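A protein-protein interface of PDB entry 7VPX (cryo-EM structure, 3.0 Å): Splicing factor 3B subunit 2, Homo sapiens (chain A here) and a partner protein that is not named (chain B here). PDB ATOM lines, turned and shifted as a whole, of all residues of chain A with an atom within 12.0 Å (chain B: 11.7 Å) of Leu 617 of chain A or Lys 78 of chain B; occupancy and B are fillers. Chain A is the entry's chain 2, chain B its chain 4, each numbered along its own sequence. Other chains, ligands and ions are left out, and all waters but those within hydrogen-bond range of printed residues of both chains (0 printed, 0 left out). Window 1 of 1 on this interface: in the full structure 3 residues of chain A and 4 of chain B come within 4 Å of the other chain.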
ATOM      1  N   LEU A 609      15.010 -18.318 -17.799  1.00  0.00           N
ATOM      2  CA  LEU A 609      14.849 -18.192 -19.241  1.00  0.00           C
ATOM      3  C   LEU A 609      15.422 -19.424 -19.929  1.00  0.00           C
ATOM      4  O   LEU A 609      16.365 -20.047 -19.437  1.00  0.00           O
ATOM      5  N   SER A 610      14.837 -19.764 -21.075  1.00  0.00           N
ATOM      6  CA  SER A 610      15.298 -20.910 -21.838  1.00  0.00           C
ATOM      7  C   SER A 610      16.600 -20.586 -22.564  1.00  0.00           C
ATOM      8  O   SER A 610      16.966 -19.422 -22.753  1.00  0.00           O
ATOM      9  N   ASP A 611      17.305 -21.644 -22.973  1.00  0.00           N
ATOM     10  CA  ASP A 611      18.572 -21.460 -23.674  1.00  0.00           C
ATOM     11  C   ASP A 611      18.361 -21.014 -25.114  1.00  0.00           C
ATOM     12  O   ASP A 611      19.170 -20.245 -25.647  1.00  0.00           O
ATOM     13  N   GLU A 612      17.281 -21.476 -25.756  1.00  0.00           N
ATOM     14  CA  GLU A 612      17.021 -21.102 -27.143  1.00  0.00           C
ATOM     15  C   GLU A 612      16.604 -19.641 -27.256  1.00  0.00           C
ATOM     16  O   GLU A 612      17.042 -18.934 -28.172  1.00  0.00           O
ATOM     17  N   LEU A 613      15.769 -19.167 -26.325  1.00  0.00           N
ATOM     18  CA  LEU A 613      15.372 -17.763 -26.329  1.00  0.00           C
ATOM     19  C   LEU A 613      16.534 -16.847 -25.970  1.00  0.00           C
ATOM     20  O   LEU A 613      16.640 -15.741 -26.512  1.00  0.00           O
ATOM     21  N   ARG A 614      17.421 -17.292 -25.075  1.00  0.00           N
ATOM     22  CA  ARG A 614      18.597 -16.497 -24.736  1.00  0.00           C
ATOM     23  C   ARG A 614      19.612 -16.490 -25.873  1.00  0.00           C
ATOM     24  O   ARG A 614      20.345 -15.507 -26.038  1.00  0.00           O
ATOM     25  N   ILE A 615      19.671 -17.564 -26.660  1.00  0.00           N
ATOM     26  CA  ILE A 615      20.566 -17.583 -27.813  1.00  0.00           C
ATOM     27  C   ILE A 615      19.998 -16.746 -28.957  1.00  0.00           C
ATOM     28  O   ILE A 615      20.757 -16.108 -29.697  1.00  0.00           O
ATOM     29  N   SER A 616      18.676 -16.734 -29.123  1.00  0.00           N
ATOM     30  CA  SER A 616      18.068 -15.943 -30.189  1.00  0.00           C
ATOM     31  C   SER A 616      18.004 -14.461 -29.844  1.00  0.00           C
ATOM     32  O   SER A 616      18.041 -13.618 -30.749  1.00  0.00           O
ATOM     33  N   LEU A 617      17.911 -14.120 -28.558  1.00  0.00           N
ATOM     34  CA  LEU A 617      17.832 -12.725 -28.146  1.00  0.00           C
ATOM     35  C   LEU A 617      19.181 -12.013 -28.181  1.00  0.00           C
ATOM     36  O   LEU A 617      19.213 -10.782 -28.099  1.00  0.00           O
ATOM     37  N   GLY A 618      20.283 -12.748 -28.293  1.00  0.00           N
ATOM     38  CA  GLY A 618      21.592 -12.126 -28.327  1.00  0.00           C
ATOM     39  C   GLY A 618      22.213 -11.892 -26.969  1.00  0.00           C
ATOM     40  O   GLY A 618      23.043 -10.990 -26.823  1.00  0.00           O
ATOM     41  N   MET A 619      21.833 -12.685 -25.963  1.00  0.00           N
ATOM     42  CA  MET A 619      22.380 -12.535 -24.620  1.00  0.00           C
ATOM     43  C   MET A 619      23.490 -13.545 -24.396  1.00  0.00           C
ATOM     44  O   MET A 619      23.294 -14.742 -24.661  1.00  0.00           O
ATOM     45  N   PRO A 620      24.659 -13.120 -23.919  1.00  0.00           N
ATOM     46  CA  PRO A 620      25.757 -14.063 -23.683  1.00  0.00           C
ATOM     47  C   PRO A 620      25.518 -14.898 -22.430  1.00  0.00           C
ATOM     48  O   PRO A 620      24.593 -14.666 -21.653  1.00  0.00           O
ATOM     49  CB  PRO A 620      26.973 -13.149 -23.516  1.00  0.00           C
ATOM     50  CG  PRO A 620      26.405 -11.875 -22.994  1.00  0.00           C
ATOM     51  CD  PRO A 620      25.055 -11.728 -23.641  1.00  0.00           C
ATOM     52  N   VAL A 621      26.393 -15.892 -22.249  1.00  0.00           N
ATOM     53  CA  VAL A 621      26.276 -16.774 -21.095  1.00  0.00           C
ATOM     54  C   VAL A 621      26.794 -16.073 -19.842  1.00  0.00           C
ATOM     55  O   VAL A 621      27.467 -15.037 -19.900  1.00  0.00           O
ATOM     56  N   PRO A 629      23.881  -8.332 -16.763  1.00  0.00           N
ATOM     57  CA  PRO A 629      22.441  -8.357 -16.519  1.00  0.00           C
ATOM     58  C   PRO A 629      21.669  -8.462 -17.822  1.00  0.00           C
ATOM     59  O   PRO A 629      22.195  -8.125 -18.896  1.00  0.00           O
ATOM     60  CB  PRO A 629      22.182  -7.008 -15.831  1.00  0.00           C
ATOM     61  CG  PRO A 629      23.202  -6.110 -16.437  1.00  0.00           C
ATOM     62  CD  PRO A 629      24.425  -6.962 -16.686  1.00  0.00           C
ATOM     63  N   PRO A 630      20.428  -8.934 -17.780  1.00  0.00           N
ATOM     64  CA  PRO A 630      19.548  -8.826 -18.948  1.00  0.00           C
ATOM     65  C   PRO A 630      19.133  -7.381 -19.165  1.00  0.00           C
ATOM     66  O   PRO A 630      19.217  -6.563 -18.239  1.00  0.00           O
ATOM     67  CB  PRO A 630      18.349  -9.711 -18.563  1.00  0.00           C
ATOM     68  CG  PRO A 630      18.353  -9.734 -17.082  1.00  0.00           C
ATOM     69  CD  PRO A 630      19.797  -9.685 -16.679  1.00  0.00           C
ATOM     70  N   PRO A 631      18.695  -7.014 -20.380  1.00  0.00           N
ATOM     71  CA  PRO A 631      18.291  -5.617 -20.620  1.00  0.00           C
ATOM     72  C   PRO A 631      17.011  -5.200 -19.909  1.00  0.00           C
ATOM     73  O   PRO A 631      16.721  -3.997 -19.858  1.00  0.00           O
ATOM     74  CB  PRO A 631      18.124  -5.556 -22.143  1.00  0.00           C
ATOM     75  CG  PRO A 631      17.849  -6.955 -22.550  1.00  0.00           C
ATOM     76  CD  PRO A 631      18.654  -7.811 -21.621  1.00  0.00           C
ATOM     77  N   TRP A 632      16.235  -6.140 -19.368  1.00  0.00           N
ATOM     78  CA  TRP A 632      15.092  -5.796 -18.533  1.00  0.00           C
ATOM     79  C   TRP A 632      15.476  -5.553 -17.081  1.00  0.00           C
ATOM     80  O   TRP A 632      14.634  -5.092 -16.302  1.00  0.00           O
ATOM     81  N   LEU A 633      16.718  -5.852 -16.695  1.00  0.00           N
ATOM     82  CA  LEU A 633      17.173  -5.648 -15.326  1.00  0.00           C
ATOM     83  C   LEU A 633      17.638  -4.223 -15.062  1.00  0.00           C
ATOM     84  O   LEU A 633      17.692  -3.804 -13.900  1.00  0.00           O
ATOM     85  N   ILE A 634      17.969  -3.468 -16.114  1.00  0.00           N
ATOM     86  CA  ILE A 634      18.382  -2.079 -15.933  1.00  0.00           C
ATOM     87  C   ILE A 634      17.200  -1.225 -15.489  1.00  0.00           C
ATOM     88  O   ILE A 634      17.347  -0.328 -14.650  1.00  0.00           O
ATOM     89  N   ALA A 635      16.007  -1.507 -16.023  1.00  0.00           N
ATOM     90  CA  ALA A 635      14.809  -0.798 -15.586  1.00  0.00           C
ATOM     91  C   ALA A 635      14.429  -1.161 -14.155  1.00  0.00           C
ATOM     92  O   ALA A 635      13.917  -0.312 -13.420  1.00  0.00           O
ATOM     93  N   GLY B  18       4.458  -6.251 -28.947  1.00  0.00           N
ATOM     94  CA  GLY B  18       4.702  -6.146 -30.375  1.00  0.00           C
ATOM     95  C   GLY B  18       6.162  -6.384 -30.690  1.00  0.00           C
ATOM     96  O   GLY B  18       7.052  -6.065 -29.897  1.00  0.00           O
ATOM     97  N   GLY B  19       6.400  -6.954 -31.867  1.00  0.00           N
ATOM     98  CA  GLY B  19       7.750  -7.260 -32.295  1.00  0.00           C
ATOM     99  C   GLY B  19       8.238  -8.607 -31.812  1.00  0.00           C
ATOM    100  O   GLY B  19       9.259  -8.695 -31.122  1.00  0.00           O
ATOM    101  N   LEU B  20       7.514  -9.669 -32.157  1.00  0.00           N
ATOM    102  CA  LEU B  20       7.871 -11.029 -31.783  1.00  0.00           C
ATOM    103  C   LEU B  20       8.317 -11.793 -33.021  1.00  0.00           C
ATOM    104  O   LEU B  20       7.632 -11.772 -34.050  1.00  0.00           O
ATOM    105  N   ASP B  21       9.460 -12.465 -32.919  1.00  0.00           N
ATOM    106  CA  ASP B  21      10.011 -13.230 -34.026  1.00  0.00           C
ATOM    107  C   ASP B  21       9.440 -14.650 -34.005  1.00  0.00           C
ATOM    108  O   ASP B  21       8.512 -14.962 -33.257  1.00  0.00           O
ATOM    109  N   GLU B  22      10.003 -15.531 -34.837  1.00  0.00           N
ATOM    110  CA  GLU B  22       9.542 -16.910 -34.901  1.00  0.00           C
ATOM    111  C   GLU B  22      10.008 -17.746 -33.716  1.00  0.00           C
ATOM    112  O   GLU B  22       9.422 -18.799 -33.450  1.00  0.00           O
ATOM    113  N   LYS B  23      11.048 -17.304 -33.003  1.00  0.00           N
ATOM    114  CA  LYS B  23      11.523 -18.058 -31.846  1.00  0.00           C
ATOM    115  C   LYS B  23      10.600 -17.887 -30.647  1.00  0.00           C
ATOM    116  O   LYS B  23      10.521 -18.783 -29.795  1.00  0.00           O
ATOM    117  N   VAL B  24       9.903 -16.752 -30.555  1.00  0.00           N
ATOM    118  CA  VAL B  24       8.973 -16.529 -29.455  1.00  0.00           C
ATOM    119  C   VAL B  24       7.704 -17.337 -29.687  1.00  0.00           C
ATOM    120  O   VAL B  24       7.242 -17.492 -30.825  1.00  0.00           O
ATOM    121  N   SER B  25       7.135 -17.859 -28.604  1.00  0.00           N
ATOM    122  CA  SER B  25       5.942 -18.688 -28.662  1.00  0.00           C
ATOM    123  C   SER B  25       4.936 -18.202 -27.624  1.00  0.00           C
ATOM    124  O   SER B  25       5.152 -17.199 -26.936  1.00  0.00           O
ATOM    125  N   LEU B  28       6.283 -19.062 -24.118  1.00  0.00           N
ATOM    126  CA  LEU B  28       7.542 -18.347 -23.926  1.00  0.00           C
ATOM    127  C   LEU B  28       7.322 -16.915 -23.458  1.00  0.00           C
ATOM    128  O   LEU B  28       8.077 -16.423 -22.610  1.00  0.00           O
ATOM    129  N   LEU B  32       8.531 -15.409 -19.929  1.00  0.00           N
ATOM    130  CA  LEU B  32       9.348 -14.201 -19.851  1.00  0.00           C
ATOM    131  C   LEU B  32       8.662 -13.104 -19.048  1.00  0.00           C
ATOM    132  O   LEU B  32       9.338 -12.298 -18.402  1.00  0.00           O
ATOM    133  N   ALA B  70       5.335  -4.534 -16.420  1.00  0.00           N
ATOM    134  CA  ALA B  70       5.796  -5.236 -17.614  1.00  0.00           C
ATOM    135  C   ALA B  70       5.930  -4.288 -18.799  1.00  0.00           C
ATOM    136  O   ALA B  70       6.796  -4.479 -19.660  1.00  0.00           O
ATOM    137  N   ILE B  73       9.147  -2.255 -18.000  1.00  0.00           N
ATOM    138  CA  ILE B  73      10.362  -3.051 -17.884  1.00  0.00           C
ATOM    139  C   ILE B  73      10.753  -3.668 -19.222  1.00  0.00           C
ATOM    140  O   ILE B  73      11.923  -3.640 -19.612  1.00  0.00           O
ATOM    141  N   MET B  74       9.785  -4.236 -19.942  1.00  0.00           N
ATOM    142  CA  MET B  74      10.042  -4.911 -21.206  1.00  0.00           C
ATOM    143  C   MET B  74       9.833  -4.003 -22.414  1.00  0.00           C
ATOM    144  O   MET B  74       9.478  -4.494 -23.491  1.00  0.00           O
ATOM    145  N   ASN B  75      10.042  -2.698 -22.260  1.00  0.00           N
ATOM    146  CA  ASN B  75       9.880  -1.752 -23.356  1.00  0.00           C
ATOM    147  C   ASN B  75      11.173  -1.659 -24.152  1.00  0.00           C
ATOM    148  O   ASN B  75      12.252  -1.490 -23.571  1.00  0.00           O
ATOM    149  N   MET B  76      11.048  -1.773 -25.483  1.00  0.00           N
ATOM    150  CA  MET B  76      12.159  -1.678 -26.445  1.00  0.00           C
ATOM    151  C   MET B  76      13.250  -2.710 -26.166  1.00  0.00           C
ATOM    152  O   MET B  76      14.444  -2.423 -26.270  1.00  0.00           O
ATOM    153  N   ILE B  77      12.838  -3.924 -25.806  1.00  0.00           N
ATOM    154  CA  ILE B  77      13.791  -4.989 -25.532  1.00  0.00           C
ATOM    155  C   ILE B  77      14.098  -5.754 -26.817  1.00  0.00           C
ATOM    156  O   ILE B  77      13.335  -5.739 -27.785  1.00  0.00           O
ATOM    157  N   LYS B  78      15.244  -6.432 -26.822  1.00  0.00           N
ATOM    158  CA  LYS B  78      15.687  -7.223 -27.969  1.00  0.00           C
ATOM    159  C   LYS B  78      15.394  -8.689 -27.665  1.00  0.00           C
ATOM    160  O   LYS B  78      16.221  -9.405 -27.097  1.00  0.00           O
ATOM    161  N   LEU B  79      14.201  -9.135 -28.047  1.00  0.00           N
ATOM    162  CA  LEU B  79      13.757 -10.505 -27.808  1.00  0.00           C
ATOM    163  C   LEU B  79      13.748 -11.252 -29.134  1.00  0.00           C
ATOM    164  O   LEU B  79      13.076 -10.825 -30.080  1.00  0.00           O
ATOM    165  N   TYR B  80      14.508 -12.355 -29.190  1.00  0.00           N
ATOM    166  CA  TYR B  80      14.645 -13.228 -30.365  1.00  0.00           C
ATOM    167  C   TYR B  80      15.130 -12.470 -31.598  1.00  0.00           C
ATOM    168  O   TYR B  80      14.734 -12.778 -32.727  1.00  0.00           O
ATOM    169  N   GLY B  81      15.997 -11.481 -31.397  1.00  0.00           N
ATOM    170  CA  GLY B  81      16.438 -10.625 -32.483  1.00  0.00           C
ATOM    171  C   GLY B  81      15.344  -9.727 -33.024  1.00  0.00           C
ATOM    172  O   GLY B  81      15.336  -9.416 -34.218  1.00  0.00           O
ATOM    173  N   LYS B  82      14.416  -9.299 -32.162  1.00  0.00           N
ATOM    174  CA  LYS B  82      13.278  -8.504 -32.589  1.00  0.00           C
ATOM    175  C   LYS B  82      12.979  -7.438 -31.545  1.00  0.00           C
ATOM    176  O   LYS B  82      13.127  -7.702 -30.342  1.00  0.00           O
ATOM    177  N   PRO B  83      12.566  -6.233 -31.965  1.00  0.00           N
ATOM    178  CA  PRO B  83      12.246  -5.185 -30.988  1.00  0.00           C
ATOM    179  C   PRO B  83      10.904  -5.403 -30.299  1.00  0.00           C
ATOM    180  O   PRO B  83       9.886  -4.821 -30.687  1.00  0.00           O
ATOM    181  CB  PRO B  83      12.243  -3.907 -31.838  1.00  0.00           C
ATOM    182  CG  PRO B  83      11.913  -4.377 -33.219  1.00  0.00           C
ATOM    183  CD  PRO B  83      12.522  -5.740 -33.351  1.00  0.00           C
ATOM    184  N   ILE B  84      10.901  -6.241 -29.262  1.00  0.00           N
ATOM    185  CA  ILE B  84       9.667  -6.514 -28.533  1.00  0.00           C
ATOM    186  C   ILE B  84       9.414  -5.403 -27.524  1.00  0.00           C
ATOM    187  O   ILE B  84      10.323  -4.972 -26.802  1.00  0.00           O
ATOM    188  N   ARG B  85       8.171  -4.936 -27.470  1.00  0.00           N
ATOM    189  CA  ARG B  85       7.791  -3.872 -26.549  1.00  0.00           C
ATOM    190  C   ARG B  85       6.356  -4.093 -26.099  1.00  0.00           C
ATOM    191  O   ARG B  85       5.503  -4.489 -26.898  1.00  0.00           O
ATOM    192  N   VAL B  86       6.098  -3.831 -24.823  1.00  0.00           N
ATOM    193  CA  VAL B  86       4.782  -4.011 -24.222  1.00  0.00           C
ATOM    194  C   VAL B  86       4.137  -2.645 -24.040  1.00  0.00           C
ATOM    195  O   VAL B  86       4.803  -1.678 -23.655  1.00  0.00           O
ATOM    196  N   ASP B 108       9.255   0.250 -35.483  1.00  0.00           N
ATOM    197  CA  ASP B 108       9.240  -0.425 -34.194  1.00  0.00           C
ATOM    198  C   ASP B 108       8.008  -0.011 -33.392  1.00  0.00           C
ATOM    199  O   ASP B 108       7.618   1.159 -33.412  1.00  0.00           O
ATOM    200  N   PRO B 109       7.373  -0.949 -32.677  1.00  0.00           N
ATOM    201  CA  PRO B 109       6.195  -0.593 -31.873  1.00  0.00           C
ATOM    202  C   PRO B 109       6.522   0.107 -30.563  1.00  0.00           C
ATOM    203  O   PRO B 109       5.592   0.538 -29.868  1.00  0.00           O
ATOM    204  CB  PRO B 109       5.534  -1.952 -31.612  1.00  0.00           C
ATOM    205  CG  PRO B 109       6.664  -2.919 -31.645  1.00  0.00           C
ATOM    206  CD  PRO B 109       7.629  -2.400 -32.677  1.00  0.00           C
ATOM    207  N   GLU B 110       7.803   0.233 -30.202  1.00  0.00           N
ATOM    208  CA  GLU B 110       8.169   0.901 -28.959  1.00  0.00           C
ATOM    209  C   GLU B 110       8.007   2.413 -29.040  1.00  0.00           C
ATOM    210  O   GLU B 110       7.889   3.066 -27.998  1.00  0.00           O
ATOM    211  N   LEU B 167      16.881   2.631 -37.154  1.00  0.00           N
ATOM    212  CA  LEU B 167      16.001   2.909 -36.027  1.00  0.00           C
ATOM    213  C   LEU B 167      16.281   1.933 -34.888  1.00  0.00           C
ATOM    214  O   LEU B 167      17.291   1.222 -34.909  1.00  0.00           O
ATOM    215  N   CYS B 168      15.394   1.895 -33.894  1.00  0.00           N
ATOM    216  CA  CYS B 168      15.585   1.028 -32.737  1.00  0.00           C
ATOM    217  C   CYS B 168      15.347  -0.433 -33.100  1.00  0.00           C
ATOM    218  O   CYS B 168      14.236  -0.948 -32.921  1.00  0.00           O
ATOM    219  N   ASN B 169      16.394  -1.083 -33.629  1.00  0.00           N
ATOM    220  CA  ASN B 169      16.412  -2.508 -33.995  1.00  0.00           C
ATOM    221  C   ASN B 169      15.338  -2.855 -35.027  1.00  0.00           C
ATOM    222  O   ASN B 169      14.771  -3.949 -35.016  1.00  0.00           O
ATOM    223  N   ARG B 170      15.063  -1.917 -35.933  1.00  0.00           N
ATOM    224  CA  ARG B 170      14.065  -2.125 -36.973  1.00  0.00           C
ATOM    225  C   ARG B 170      14.380  -1.254 -38.185  1.00  0.00           C
ATOM    226  O   ARG B 170      14.314  -0.022 -38.094  1.00  0.00           O
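O of Leu 617 of chain A lies close to O of Lys 78 of chain B (3.4 Å). The backbone carbonyl oxygen (O) of Ser 616 of chain A lies within hydrogen-bond range of the backbone NH (N) of Gly 81 of chain B.
Among the printed residues, pairs that only touch across the chains: Ser 616 of chain A with Tyr 80 of chain B, Leu 617 of chain A with Tyr 80 of chain B, Leu 617 of chain A with Gly 81 of chain B and Trp 632 of chain A with Ile 73 of chain B.
Ser 610 of chain A touches none of the printed residues of chain B. No residue of chain B comes within 4 Å of Leu 613 of chain A. No residue of chain B comes within 4 Å of Arg 614 of chain A. No residue of chain B comes within 4 Å of Ile 615 of chain A. Of chain B, only Lys 78 (3.4 Å), Tyr 80 (3.5 Å) and Gly 81 (3.9 Å) come within 4 Å of Leu 617 of chain A. No residue of chain B comes within 4 Å of Gly 618 of chain A. No residue of chain B comes within 4 Å of Met 619 of chain A. Pro 631 of chain A touches none of the printed residues of chain B. Of the printed residues of chain B, Trp 632 of chain A touches Ile 73 (3.98 Å). Printed residues of chain A within 4 Å of Ile 73 of chain B: Trp 632. No residue of chain A comes within 4 Å of Met 76 of chain B. No residue of chain A comes within 4 Å of Ile 77 of chain B. Lys 78 of chain B touches just one residue of chain A: Leu 617 (3.4 Å). No residue of chain A comes within 4 Å of Leu 79 of chain B. Tyr 80 of chain B touches two residues of chain A. No residue of chain A comes within 4 Å of Lys 82 of chain B. No residue of chain A comes within 4 Å of Ile 84 of chain B. Glu 110 of chain B touches none of the printed residues of chain A. The nearest residue of chain B that does not touch Leu 617 of chain A is Leu 79 of chain B (4.5 Å). The nearest residue of chain A that does not touch Lys 78 of chain B is Pro 631 of chain A (5.0 Å). The nearest printed residue of chain A that does not touch Ile 73 of chain B is Pro 631 of chain A (4.8 Å).
Of the 20 printed residues of chain A, 3 touch a printed residue of chain B. Printed residues of chain B that touch a printed residue of chain A: Ile 73, Lys 78, Tyr 80 and Gly 81. Along chain B the printed residues that touch a printed residue of chain A span positions 73 to 81. Among the printed residues, 6 pairs touch across the chains. Among the printed residues, no Asp or Glu carboxylate lies within 4 Å of a Lys or Arg side-chain nitrogen of the other chain.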
